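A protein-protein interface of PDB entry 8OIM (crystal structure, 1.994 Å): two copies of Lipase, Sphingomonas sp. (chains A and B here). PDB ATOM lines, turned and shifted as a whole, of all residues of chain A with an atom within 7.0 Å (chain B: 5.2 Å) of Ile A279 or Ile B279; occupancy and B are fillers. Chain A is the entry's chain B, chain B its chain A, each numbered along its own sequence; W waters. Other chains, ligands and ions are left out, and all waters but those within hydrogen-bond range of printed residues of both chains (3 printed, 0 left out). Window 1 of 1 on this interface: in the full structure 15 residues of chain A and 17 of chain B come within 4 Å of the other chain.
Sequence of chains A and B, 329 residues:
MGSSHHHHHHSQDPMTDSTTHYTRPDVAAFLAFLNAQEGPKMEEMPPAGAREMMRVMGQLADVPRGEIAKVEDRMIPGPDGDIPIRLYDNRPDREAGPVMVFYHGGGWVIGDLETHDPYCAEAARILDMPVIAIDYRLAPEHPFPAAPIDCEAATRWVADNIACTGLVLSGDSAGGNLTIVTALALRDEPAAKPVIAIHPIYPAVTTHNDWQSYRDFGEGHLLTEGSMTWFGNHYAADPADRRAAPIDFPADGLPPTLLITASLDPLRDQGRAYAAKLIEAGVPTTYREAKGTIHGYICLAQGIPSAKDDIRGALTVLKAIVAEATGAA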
ATOM      1  N   ALA A 251       0.528  15.252  27.545  1.00  0.00           N
ATOM      2  CA  ALA A 251       0.518  16.692  27.793  1.00  0.00           C
ATOM      3  C   ALA A 251      -0.030  17.434  26.578  1.00  0.00           C
ATOM      4  O   ALA A 251      -0.148  18.638  26.614  1.00  0.00           O
ATOM      5  CB  ALA A 251       1.929  17.140  28.116  1.00  0.00           C
ATOM      6  N   GLY A 271      10.932  19.301  37.245  1.00  0.00           N
ATOM      7  CA  GLY A 271      10.402  20.498  36.607  1.00  0.00           C
ATOM      8  C   GLY A 271      10.910  20.624  35.169  1.00  0.00           C
ATOM      9  O   GLY A 271      10.122  20.882  34.262  1.00  0.00           O
ATOM     10  N   ARG A 272      12.248  20.523  34.992  1.00  0.00           N
ATOM     11  CA  ARG A 272      12.857  20.508  33.674  1.00  0.00           C
ATOM     12  C   ARG A 272      12.232  19.405  32.837  1.00  0.00           C
ATOM     13  O   ARG A 272      11.946  19.585  31.662  1.00  0.00           O
ATOM     14  CB  ARG A 272      14.368  20.260  33.772  1.00  0.00           C
ATOM     15  CG  ARG A 272      15.168  21.445  34.291  1.00  0.00           C
ATOM     16  CD  ARG A 272      16.629  21.079  34.369  1.00  0.00           C
ATOM     17  NE  ARG A 272      17.453  22.142  34.923  1.00  0.00           N
ATOM     18  CZ  ARG A 272      18.753  22.020  35.139  1.00  0.00           C
ATOM     19  NH1 ARG A 272      19.315  20.877  34.930  1.00  0.00           N
ATOM     20  NH2 ARG A 272      19.458  23.017  35.622  1.00  0.00           N
ATOM     21  N   ALA A 273      12.080  18.212  33.424  1.00  0.00           N
ATOM     22  CA  ALA A 273      11.590  17.112  32.628  1.00  0.00           C
ATOM     23  C   ALA A 273      10.152  17.333  32.161  1.00  0.00           C
ATOM     24  O   ALA A 273       9.775  17.013  31.008  1.00  0.00           O
ATOM     25  CB  ALA A 273      11.780  15.829  33.378  1.00  0.00           C
ATOM     26  N   TYR A 274       9.357  17.945  32.994  1.00  0.00           N
ATOM     27  CA  TYR A 274       7.999  18.288  32.575  1.00  0.00           C
ATOM     28  C   TYR A 274       7.965  19.349  31.484  1.00  0.00           C
ATOM     29  O   TYR A 274       7.153  19.243  30.567  1.00  0.00           O
ATOM     30  CB  TYR A 274       7.082  18.698  33.729  1.00  0.00           C
ATOM     31  CG  TYR A 274       5.620  18.583  33.339  1.00  0.00           C
ATOM     32  CD1 TYR A 274       4.977  17.362  33.317  1.00  0.00           C
ATOM     33  CD2 TYR A 274       4.863  19.699  33.004  1.00  0.00           C
ATOM     34  CE1 TYR A 274       3.659  17.227  32.960  1.00  0.00           C
ATOM     35  CE2 TYR A 274       3.543  19.570  32.595  1.00  0.00           C
ATOM     36  CZ  TYR A 274       2.970  18.330  32.485  1.00  0.00           C
ATOM     37  OH  TYR A 274       1.660  18.127  32.080  1.00  0.00           O
ATOM     38  N   ALA A 275       8.787  20.378  31.571  1.00  0.00           N
ATOM     39  CA  ALA A 275       8.853  21.407  30.581  1.00  0.00           C
ATOM     40  C   ALA A 275       9.303  20.788  29.262  1.00  0.00           C
ATOM     41  O   ALA A 275       8.757  21.130  28.193  1.00  0.00           O
ATOM     42  CB  ALA A 275       9.752  22.560  31.045  1.00  0.00           C
ATOM     43  N   ALA A 276      10.234  19.838  29.323  1.00  0.00           N
ATOM     44  CA  ALA A 276      10.707  19.174  28.111  1.00  0.00           C
ATOM     45  C   ALA A 276       9.606  18.292  27.476  1.00  0.00           C
ATOM     46  O   ALA A 276       9.464  18.139  26.236  1.00  0.00           O
ATOM     47  CB  ALA A 276      11.960  18.384  28.433  1.00  0.00           C
ATOM     48  N   LYS A 277       8.784  17.663  28.304  1.00  0.00           N
ATOM     49  CA  LYS A 277       7.652  16.868  27.803  1.00  0.00           C
ATOM     50  C   LYS A 277       6.603  17.726  27.097  1.00  0.00           C
ATOM     51  O   LYS A 277       5.996  17.337  26.107  1.00  0.00           O
ATOM     52  CB  LYS A 277       7.061  16.193  29.004  1.00  0.00           C
ATOM     53  CG  LYS A 277       5.870  15.282  28.785  1.00  0.00           C
ATOM     54  CD  LYS A 277       5.176  15.022  30.131  1.00  0.00           C
ATOM     55  CE  LYS A 277       3.840  14.380  29.906  1.00  0.00           C
ATOM     56  NZ  LYS A 277       4.040  13.001  29.377  1.00  0.00           N
ATOM     57  N   LEU A 278       6.402  18.938  27.612  1.00  0.00           N
ATOM     58  CA  LEU A 278       5.462  19.882  27.043  1.00  0.00           C
ATOM     59  C   LEU A 278       5.944  20.279  25.660  1.00  0.00           C
ATOM     60  O   LEU A 278       5.099  20.274  24.741  1.00  0.00           O
ATOM     61  CB  LEU A 278       5.285  21.107  27.924  1.00  0.00           C
ATOM     62  CG  LEU A 278       4.467  20.894  29.191  1.00  0.00           C
ATOM     63  CD1 LEU A 278       4.588  22.120  30.078  1.00  0.00           C
ATOM     64  CD2 LEU A 278       3.009  20.733  28.866  1.00  0.00           C
ATOM     65  N   ILE A 279       7.247  20.614  25.529  1.00  0.00           N
ATOM     66  CA  ILE A 279       7.801  20.994  24.242  1.00  0.00           C
ATOM     67  C   ILE A 279       7.668  19.833  23.259  1.00  0.00           C
ATOM     68  O   ILE A 279       7.252  20.024  22.116  1.00  0.00           O
ATOM     69  CB  ILE A 279       9.272  21.419  24.405  1.00  0.00           C
ATOM     70  CG1 ILE A 279       9.346  22.752  25.130  1.00  0.00           C
ATOM     71  CG2 ILE A 279       9.971  21.435  23.047  1.00  0.00           C
ATOM     72  CD1 ILE A 279      10.621  23.371  25.221  1.00  0.00           C
ATOM     73  N   GLU A 280       7.999  18.619  23.695  1.00  0.00           N
ATOM     74  CA  GLU A 280       7.864  17.459  22.842  1.00  0.00           C
ATOM     75  C   GLU A 280       6.435  17.192  22.398  1.00  0.00           C
ATOM     76  O   GLU A 280       6.301  16.629  21.357  1.00  0.00           O
ATOM     77  CB  GLU A 280       8.480  16.211  23.456  1.00  0.00           C
ATOM     78  CG  GLU A 280       9.967  16.353  23.739  1.00  0.00           C
ATOM     79  CD  GLU A 280      10.917  16.058  22.586  1.00  0.00           C
ATOM     80  OE1 GLU A 280      10.452  16.171  21.417  1.00  0.00           O
ATOM     81  OE2 GLU A 280      12.108  15.659  22.879  1.00  0.00           O
ATOM     82  N   ALA A 281       5.410  17.595  23.130  1.00  0.00           N
ATOM     83  CA  ALA A 281       4.025  17.525  22.695  1.00  0.00           C
ATOM     84  C   ALA A 281       3.583  18.768  21.904  1.00  0.00           C
ATOM     85  O   ALA A 281       2.427  18.955  21.627  1.00  0.00           O
ATOM     86  CB  ALA A 281       3.167  17.358  23.942  1.00  0.00           C
ATOM     87  N   GLY A 282       4.471  19.708  21.601  1.00  0.00           N
ATOM     88  CA  GLY A 282       4.049  20.838  20.797  1.00  0.00           C
ATOM     89  C   GLY A 282       3.402  21.982  21.609  1.00  0.00           C
ATOM     90  O   GLY A 282       2.879  22.939  21.050  1.00  0.00           O
ATOM     91  N   VAL A 283       3.475  21.946  22.932  1.00  0.00           N
ATOM     92  CA  VAL A 283       2.895  23.001  23.756  1.00  0.00           C
ATOM     93  C   VAL A 283       3.861  24.169  23.817  1.00  0.00           C
ATOM     94  O   VAL A 283       4.975  24.019  24.286  1.00  0.00           O
ATOM     95  CB  VAL A 283       2.555  22.463  25.155  1.00  0.00           C
ATOM     96  CG1 VAL A 283       1.964  23.547  26.051  1.00  0.00           C
ATOM     97  CG2 VAL A 283       1.618  21.273  25.038  1.00  0.00           C
ATOM     98  N   PRO A 284       3.485  25.382  23.405  1.00  0.00           N
ATOM     99  CA  PRO A 284       4.353  26.560  23.568  1.00  0.00           C
ATOM    100  C   PRO A 284       4.730  26.770  25.035  1.00  0.00           C
ATOM    101  O   PRO A 284       3.872  26.723  25.913  1.00  0.00           O
ATOM    102  CB  PRO A 284       3.497  27.740  23.090  1.00  0.00           C
ATOM    103  CG  PRO A 284       2.402  27.099  22.295  1.00  0.00           C
ATOM    104  CD  PRO A 284       2.169  25.728  22.862  1.00  0.00           C
ATOM    105  N   THR A 285       6.013  26.839  25.322  1.00  0.00           N
ATOM    106  CA  THR A 285       6.510  26.749  26.695  1.00  0.00           C
ATOM    107  C   THR A 285       7.625  27.774  26.886  1.00  0.00           C
ATOM    108  O   THR A 285       8.478  27.908  26.007  1.00  0.00           O
ATOM    109  CB  THR A 285       7.030  25.321  27.040  1.00  0.00           C
ATOM    110  OG1 THR A 285       5.934  24.412  26.910  1.00  0.00           O
ATOM    111  CG2 THR A 285       7.654  25.134  28.425  1.00  0.00           C
ATOM    112  N   THR A 286       7.611  28.461  28.018  1.00  0.00           N
ATOM    113  CA  THR A 286       8.740  29.276  28.400  1.00  0.00           C
ATOM    114  C   THR A 286       9.273  28.683  29.675  1.00  0.00           C
ATOM    115  O   THR A 286       8.511  28.549  30.630  1.00  0.00           O
ATOM    116  CB  THR A 286       8.327  30.744  28.584  1.00  0.00           C
ATOM    117  OG1 THR A 286       7.758  31.287  27.412  1.00  0.00           O
ATOM    118  CG2 THR A 286       9.464  31.634  28.999  1.00  0.00           C
ATOM    119  N   TYR A 287      10.554  28.327  29.636  1.00  0.00           N
ATOM    120  CA  TYR A 287      11.224  27.776  30.796  1.00  0.00           C
ATOM    121  C   TYR A 287      12.133  28.860  31.356  1.00  0.00           C
ATOM    122  O   TYR A 287      13.030  29.343  30.661  1.00  0.00           O
ATOM    123  CB  TYR A 287      11.942  26.477  30.459  1.00  0.00           C
ATOM    124  CG  TYR A 287      12.801  25.937  31.562  1.00  0.00           C
ATOM    125  CD1 TYR A 287      12.176  25.398  32.653  1.00  0.00           C
ATOM    126  CD2 TYR A 287      14.185  26.100  31.593  1.00  0.00           C
ATOM    127  CE1 TYR A 287      12.895  24.971  33.733  1.00  0.00           C
ATOM    128  CE2 TYR A 287      14.927  25.667  32.681  1.00  0.00           C
ATOM    129  CZ  TYR A 287      14.260  25.138  33.773  1.00  0.00           C
ATOM    130  OH  TYR A 287      14.775  24.648  34.953  1.00  0.00           O
ATOM    131  N   ARG A 288      11.989  29.092  32.643  1.00  0.00           N
ATOM    132  CA  ARG A 288      12.874  30.015  33.353  1.00  0.00           C
ATOM    133  C   ARG A 288      13.493  29.261  34.536  1.00  0.00           C
ATOM    134  O   ARG A 288      12.860  28.440  35.170  1.00  0.00           O
ATOM    135  CB  ARG A 288      12.147  31.274  33.839  1.00  0.00           C
ATOM    136  CG  ARG A 288      11.640  32.179  32.716  1.00  0.00           C
ATOM    137  CD  ARG A 288      10.781  33.312  33.222  1.00  0.00           C
ATOM    138  NE  ARG A 288      11.534  34.292  34.019  1.00  0.00           N
ATOM    139  CZ  ARG A 288      12.271  35.275  33.537  1.00  0.00           C
ATOM    140  NH1 ARG A 288      12.404  35.451  32.228  1.00  0.00           N
ATOM    141  NH2 ARG A 288      12.835  36.103  34.396  1.00  0.00           N
ATOM    142  N   GLU A 289      14.768  29.503  34.820  1.00  0.00           N
ATOM    143  CA  GLU A 289      15.364  28.890  35.980  1.00  0.00           C
ATOM    144  C   GLU A 289      15.903  30.033  36.832  1.00  0.00           C
ATOM    145  O   GLU A 289      16.678  30.858  36.358  1.00  0.00           O
ATOM    146  CB  GLU A 289      16.411  27.849  35.626  1.00  0.00           C
ATOM    147  CG  GLU A 289      16.866  26.966  36.806  1.00  0.00           C
ATOM    148  CD  GLU A 289      17.683  25.763  36.301  1.00  0.00           C
ATOM    149  OE1 GLU A 289      17.118  24.814  35.550  1.00  0.00           O
ATOM    150  OE2 GLU A 289      18.910  25.751  36.642  1.00  0.00           O
ATOM    151  N   ARG B 272      11.906  20.678  18.171  1.00  0.00           N
ATOM    152  CA  ARG B 272      11.367  20.338  19.489  1.00  0.00           C
ATOM    153  C   ARG B 272      12.408  19.613  20.339  1.00  0.00           C
ATOM    154  O   ARG B 272      12.576  19.848  21.551  1.00  0.00           O
ATOM    155  CB  ARG B 272      10.100  19.490  19.388  1.00  0.00           C
ATOM    156  CG  ARG B 272       8.895  20.249  18.852  1.00  0.00           C
ATOM    157  CD  ARG B 272       7.743  19.272  18.824  1.00  0.00           C
ATOM    158  NE  ARG B 272       6.510  19.859  18.330  1.00  0.00           N
ATOM    159  CZ  ARG B 272       5.426  19.157  18.075  1.00  0.00           C
ATOM    160  NH1 ARG B 272       5.469  17.861  18.189  1.00  0.00           N
ATOM    161  NH2 ARG B 272       4.328  19.732  17.641  1.00  0.00           N
ATOM    162  N   ALA B 275      15.069  22.034  21.643  1.00  0.00           N
ATOM    163  CA  ALA B 275      14.561  22.920  22.649  1.00  0.00           C
ATOM    164  C   ALA B 275      14.457  22.144  23.957  1.00  0.00           C
ATOM    165  O   ALA B 275      14.855  22.685  24.998  1.00  0.00           O
ATOM    166  CB  ALA B 275      13.230  23.492  22.215  1.00  0.00           C
ATOM    167  N   ALA B 276      14.020  20.866  23.893  1.00  0.00           N
ATOM    168  CA  ALA B 276      13.922  20.011  25.071  1.00  0.00           C
ATOM    169  C   ALA B 276      15.280  19.763  25.718  1.00  0.00           C
ATOM    170  O   ALA B 276      15.408  19.717  26.962  1.00  0.00           O
ATOM    171  CB  ALA B 276      13.234  18.708  24.736  1.00  0.00           C
ATOM    172  N   LYS B 277      16.296  19.559  24.885  1.00  0.00           N
ATOM    173  CA  LYS B 277      17.620  19.273  25.411  1.00  0.00           C
ATOM    174  C   LYS B 277      18.218  20.489  26.110  1.00  0.00           C
ATOM    175  O   LYS B 277      18.917  20.326  27.122  1.00  0.00           O
ATOM    176  CB  LYS B 277      18.446  18.768  24.218  1.00  0.00           C
ATOM    177  CG  LYS B 277      19.944  18.597  24.353  1.00  0.00           C
ATOM    178  CD  LYS B 277      20.510  18.358  22.970  1.00  0.00           C
ATOM    179  CE  LYS B 277      22.010  18.316  22.888  1.00  0.00           C
ATOM    180  NZ  LYS B 277      22.594  17.321  23.784  1.00  0.00           N
ATOM    181  N   LEU B 278      17.907  21.689  25.615  1.00  0.00           N
ATOM    182  CA  LEU B 278      18.297  22.936  26.217  1.00  0.00           C
ATOM    183  C   LEU B 278      17.678  23.055  27.607  1.00  0.00           C
ATOM    184  O   LEU B 278      18.414  23.398  28.513  1.00  0.00           O
ATOM    185  CB  LEU B 278      17.885  24.163  25.391  1.00  0.00           C
ATOM    186  CG  LEU B 278      18.688  24.351  24.106  1.00  0.00           C
ATOM    187  CD1 LEU B 278      17.948  25.256  23.159  1.00  0.00           C
ATOM    188  CD2 LEU B 278      20.067  24.883  24.402  1.00  0.00           C
ATOM    189  N   ILE B 279      16.377  22.769  27.748  1.00  0.00           N
ATOM    190  CA  ILE B 279      15.732  22.786  29.031  1.00  0.00           C
ATOM    191  C   ILE B 279      16.340  21.763  30.004  1.00  0.00           C
ATOM    192  O   ILE B 279      16.636  22.056  31.170  1.00  0.00           O
ATOM    193  CB  ILE B 279      14.230  22.577  28.848  1.00  0.00           C
ATOM    194  CG1 ILE B 279      13.607  23.748  28.127  1.00  0.00           C
ATOM    195  CG2 ILE B 279      13.565  22.409  30.208  1.00  0.00           C
ATOM    196  CD1 ILE B 279      12.118  23.809  28.237  1.00  0.00           C
ATOM    197  N   GLU B 280      16.573  20.554  29.524  1.00  0.00           N
ATOM    198  CA  GLU B 280      17.217  19.546  30.352  1.00  0.00           C
ATOM    199  C   GLU B 280      18.651  19.924  30.782  1.00  0.00           C
ATOM    200  O   GLU B 280      19.102  19.441  31.809  1.00  0.00           O
ATOM    201  CB  GLU B 280      17.201  18.162  29.731  1.00  0.00           C
ATOM    202  CG  GLU B 280      15.812  17.516  29.574  1.00  0.00           C
ATOM    203  CD  GLU B 280      15.794  16.623  28.302  1.00  0.00           C
ATOM    204  OE1 GLU B 280      16.878  16.444  27.681  1.00  0.00           O
ATOM    205  OE2 GLU B 280      14.714  16.142  27.828  1.00  0.00           O
ATOM    206  N   ALA B 281      19.336  20.790  30.080  1.00  0.00           N
ATOM    207  CA  ALA B 281      20.654  21.303  30.470  1.00  0.00           C
ATOM    208  C   ALA B 281      20.522  22.581  31.297  1.00  0.00           C
ATOM    209  O   ALA B 281      21.512  23.229  31.642  1.00  0.00           O
ATOM    210  CB  ALA B 281      21.478  21.531  29.244  1.00  0.00           C
ATOM    211  N   GLY B 282      19.312  23.008  31.635  1.00  0.00           N
ATOM    212  CA  GLY B 282      19.158  24.225  32.437  1.00  0.00           C
ATOM    213  C   GLY B 282      19.299  25.558  31.662  1.00  0.00           C
ATOM    214  O   GLY B 282      19.510  26.618  32.256  1.00  0.00           O
ATOM    215  N   VAL B 283      19.264  25.549  30.327  1.00  0.00           N
ATOM    216  CA  VAL B 283      19.328  26.806  29.569  1.00  0.00           C
ATOM    217  C   VAL B 283      17.942  27.465  29.547  1.00  0.00           C
ATOM    218  O   VAL B 283      16.978  26.834  29.169  1.00  0.00           O
ATOM    219  CB  VAL B 283      19.826  26.533  28.135  1.00  0.00           C
ATOM    220  CG1 VAL B 283      19.761  27.741  27.249  1.00  0.00           C
ATOM    221  CG2 VAL B 283      21.231  25.925  28.171  1.00  0.00           C
ATOM    222  N   THR B 285      14.797  28.942  28.102  1.00  0.00           N
ATOM    223  CA  THR B 285      14.382  28.652  26.741  1.00  0.00           C
ATOM    224  C   THR B 285      12.935  29.068  26.607  1.00  0.00           C
ATOM    225  O   THR B 285      12.108  28.785  27.488  1.00  0.00           O
ATOM    226  CB  THR B 285      14.571  27.156  26.352  1.00  0.00           C
ATOM    227  OG1 THR B 285      15.975  26.921  26.376  1.00  0.00           O
ATOM    228  CG2 THR B 285      14.090  26.739  24.963  1.00  0.00           C
ATOM    229  N   TYR B 287      10.152  28.323  23.776  1.00  0.00           N
ATOM    230  CA  TYR B 287       9.795  27.577  22.589  1.00  0.00           C
ATOM    231  C   TYR B 287       8.471  28.112  22.075  1.00  0.00           C
ATOM    232  O   TYR B 287       7.462  28.095  22.803  1.00  0.00           O
ATOM    233  CB  TYR B 287       9.704  26.093  22.961  1.00  0.00           C
ATOM    234  CG  TYR B 287       9.170  25.243  21.851  1.00  0.00           C
ATOM    235  CD1 TYR B 287       9.933  25.105  20.713  1.00  0.00           C
ATOM    236  CD2 TYR B 287       7.857  24.758  21.831  1.00  0.00           C
ATOM    237  CE1 TYR B 287       9.449  24.435  19.631  1.00  0.00           C
ATOM    238  CE2 TYR B 287       7.355  24.100  20.721  1.00  0.00           C
ATOM    239  CZ  TYR B 287       8.175  23.944  19.627  1.00  0.00           C
ATOM    240  OH  TYR B 287       7.866  23.305  18.482  1.00  0.00           O
HETATM  241  O   HOH W   1       8.016  15.910  19.023  1.00  0.00           O
HETATM  242  O   HOH W   2      13.114  31.673  29.490  1.00  0.00           O
HETATM  243  O   HOH W   3      18.095  18.026  34.176  1.00  0.00           O
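O of Leu B278 is in hydrogen-bond range of N of Val B283. O of Val B283 sits at hydrogen-bond distance from OG1 of Thr B285 (3.0 Å). The side-chain carboxylate of Glu A289 is in salt-bridge range of the guanidinium group of Arg A272, 2.8 Å away. The backbone NH (N) of Val A283 lies within hydrogen-bond range of the backbone carbonyl oxygen (O) of Leu A278 (3.0 Å). The side-chain carboxylate (OE1) of Glu A289 sits at hydrogen-bond distance from the side-chain hydroxyl (OH) of Tyr A287 (2.4 Å). The side-chain hydroxyl (OG1) of Thr A285 lies within hydrogen-bond range of the backbone carbonyl oxygen (O) of Val A283, at 2.8 Å.
Water W2 lies within hydrogen-bond range of the backbone carbonyl oxygen of Tyr A287 and the backbone NH of Thr B285. Water W3 lies within hydrogen-bond range of the backbone carbonyl oxygen of Glu B280 and the guanidinium group of Arg A272. Water W1 bridges the backbone carbonyl oxygen (O) of Glu A280 (3.0 Å) and the guanidinium group (NH1) of Arg B272 (3.3 Å).
Hydrophobic or aromatic side chains of chain B within 4 Å of the printed part of chain A: Ala B275, Ala B276, Ile B279 and Tyr B287. Of the 20 printed residues of chain A, 12 touch a printed residue of chain B. Among the printed residues, 21 pairs touch across the chains. Among the printed residues, no Asp or Glu carboxylate lies within 4 Å of a Lys or Arg side-chain nitrogen of the other chain.
The guanidinium group (NH1) of Arg A272 lies within hydrogen-bond range of the backbone carbonyl oxygen (O) of Glu B280. The backbone NH of Tyr A287 lies within hydrogen-bond range of the backbone carbonyl oxygen of Thr B285 (2.7 Å). The backbone carbonyl oxygen (O) of Glu A280 lies close to the guanidinium group (NH1) of Arg B272 (3.5 Å). The backbone carbonyl oxygen (O) of Thr A285 sits at hydrogen-bond distance from the backbone NH (N) of Tyr B287.
Of the printed residues of chain B, Ala A276 touches Ala B276 (3.9 Å) and Glu B280 (3.6 Å). Ile A279 touches just these residues of chain B: Arg B272, Ala B275, Ile B279 and Tyr B287. Ala A281 touches none of the printed residues of chain B. Leu B278 touches none of the printed residues of chain A. Ile B279 touches four residues of chain A. Printed residues of chain A within 4 Å of Thr B285: Thr A286 and Tyr A287. The nearest residue of chain B that does not touch Ile A279 is Ala B276 (4.2 Å). The nearest residue of chain A that does not touch Ile B279 is Ala A276 (4.3 Å).
Arg A272 touches Ile B279, and with the chains exchanged Ile A279 touches Arg B272. Arg A272 touches Gly B282, and with the chains exchanged Gly A282 touches Arg B272. Ala A275 touches Ile B279, and with the chains exchanged Ile A279 touches Ala B275. Ala A276 touches Glu B280, and with the chains exchanged Glu A280 touches Ala B276. Of the 21 pairs that touch across the chains among the printed residues, 18 have their exchanged pair printed and touching as well.
NH2 of Arg A272 touches CA of Gly B282 (3.4 Å). Ala A275 touches Ile B279 (CB to CD1, 3.9 Å). Ala A276 touches Glu B280 (CB to OE2, 3.6 Å). CG2 of Ile A279 touches CB of Ala B275, at 3.9 Å. CD1 of Ile A279 touches CD1 of Ile B279, at 3.4 Å. Gly A282 touches Arg B272 (CA to NH2, 3.4 Å). CA of Pro A284 touches O of Tyr B287, 3.6 Å away. Ile B279 touches Tyr A287 (CD1 to CB, 3.5 Å). Val B283 touches Tyr A287. Glu A289 touches Gly B282 (OE1 to CA, 3.8 Å).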
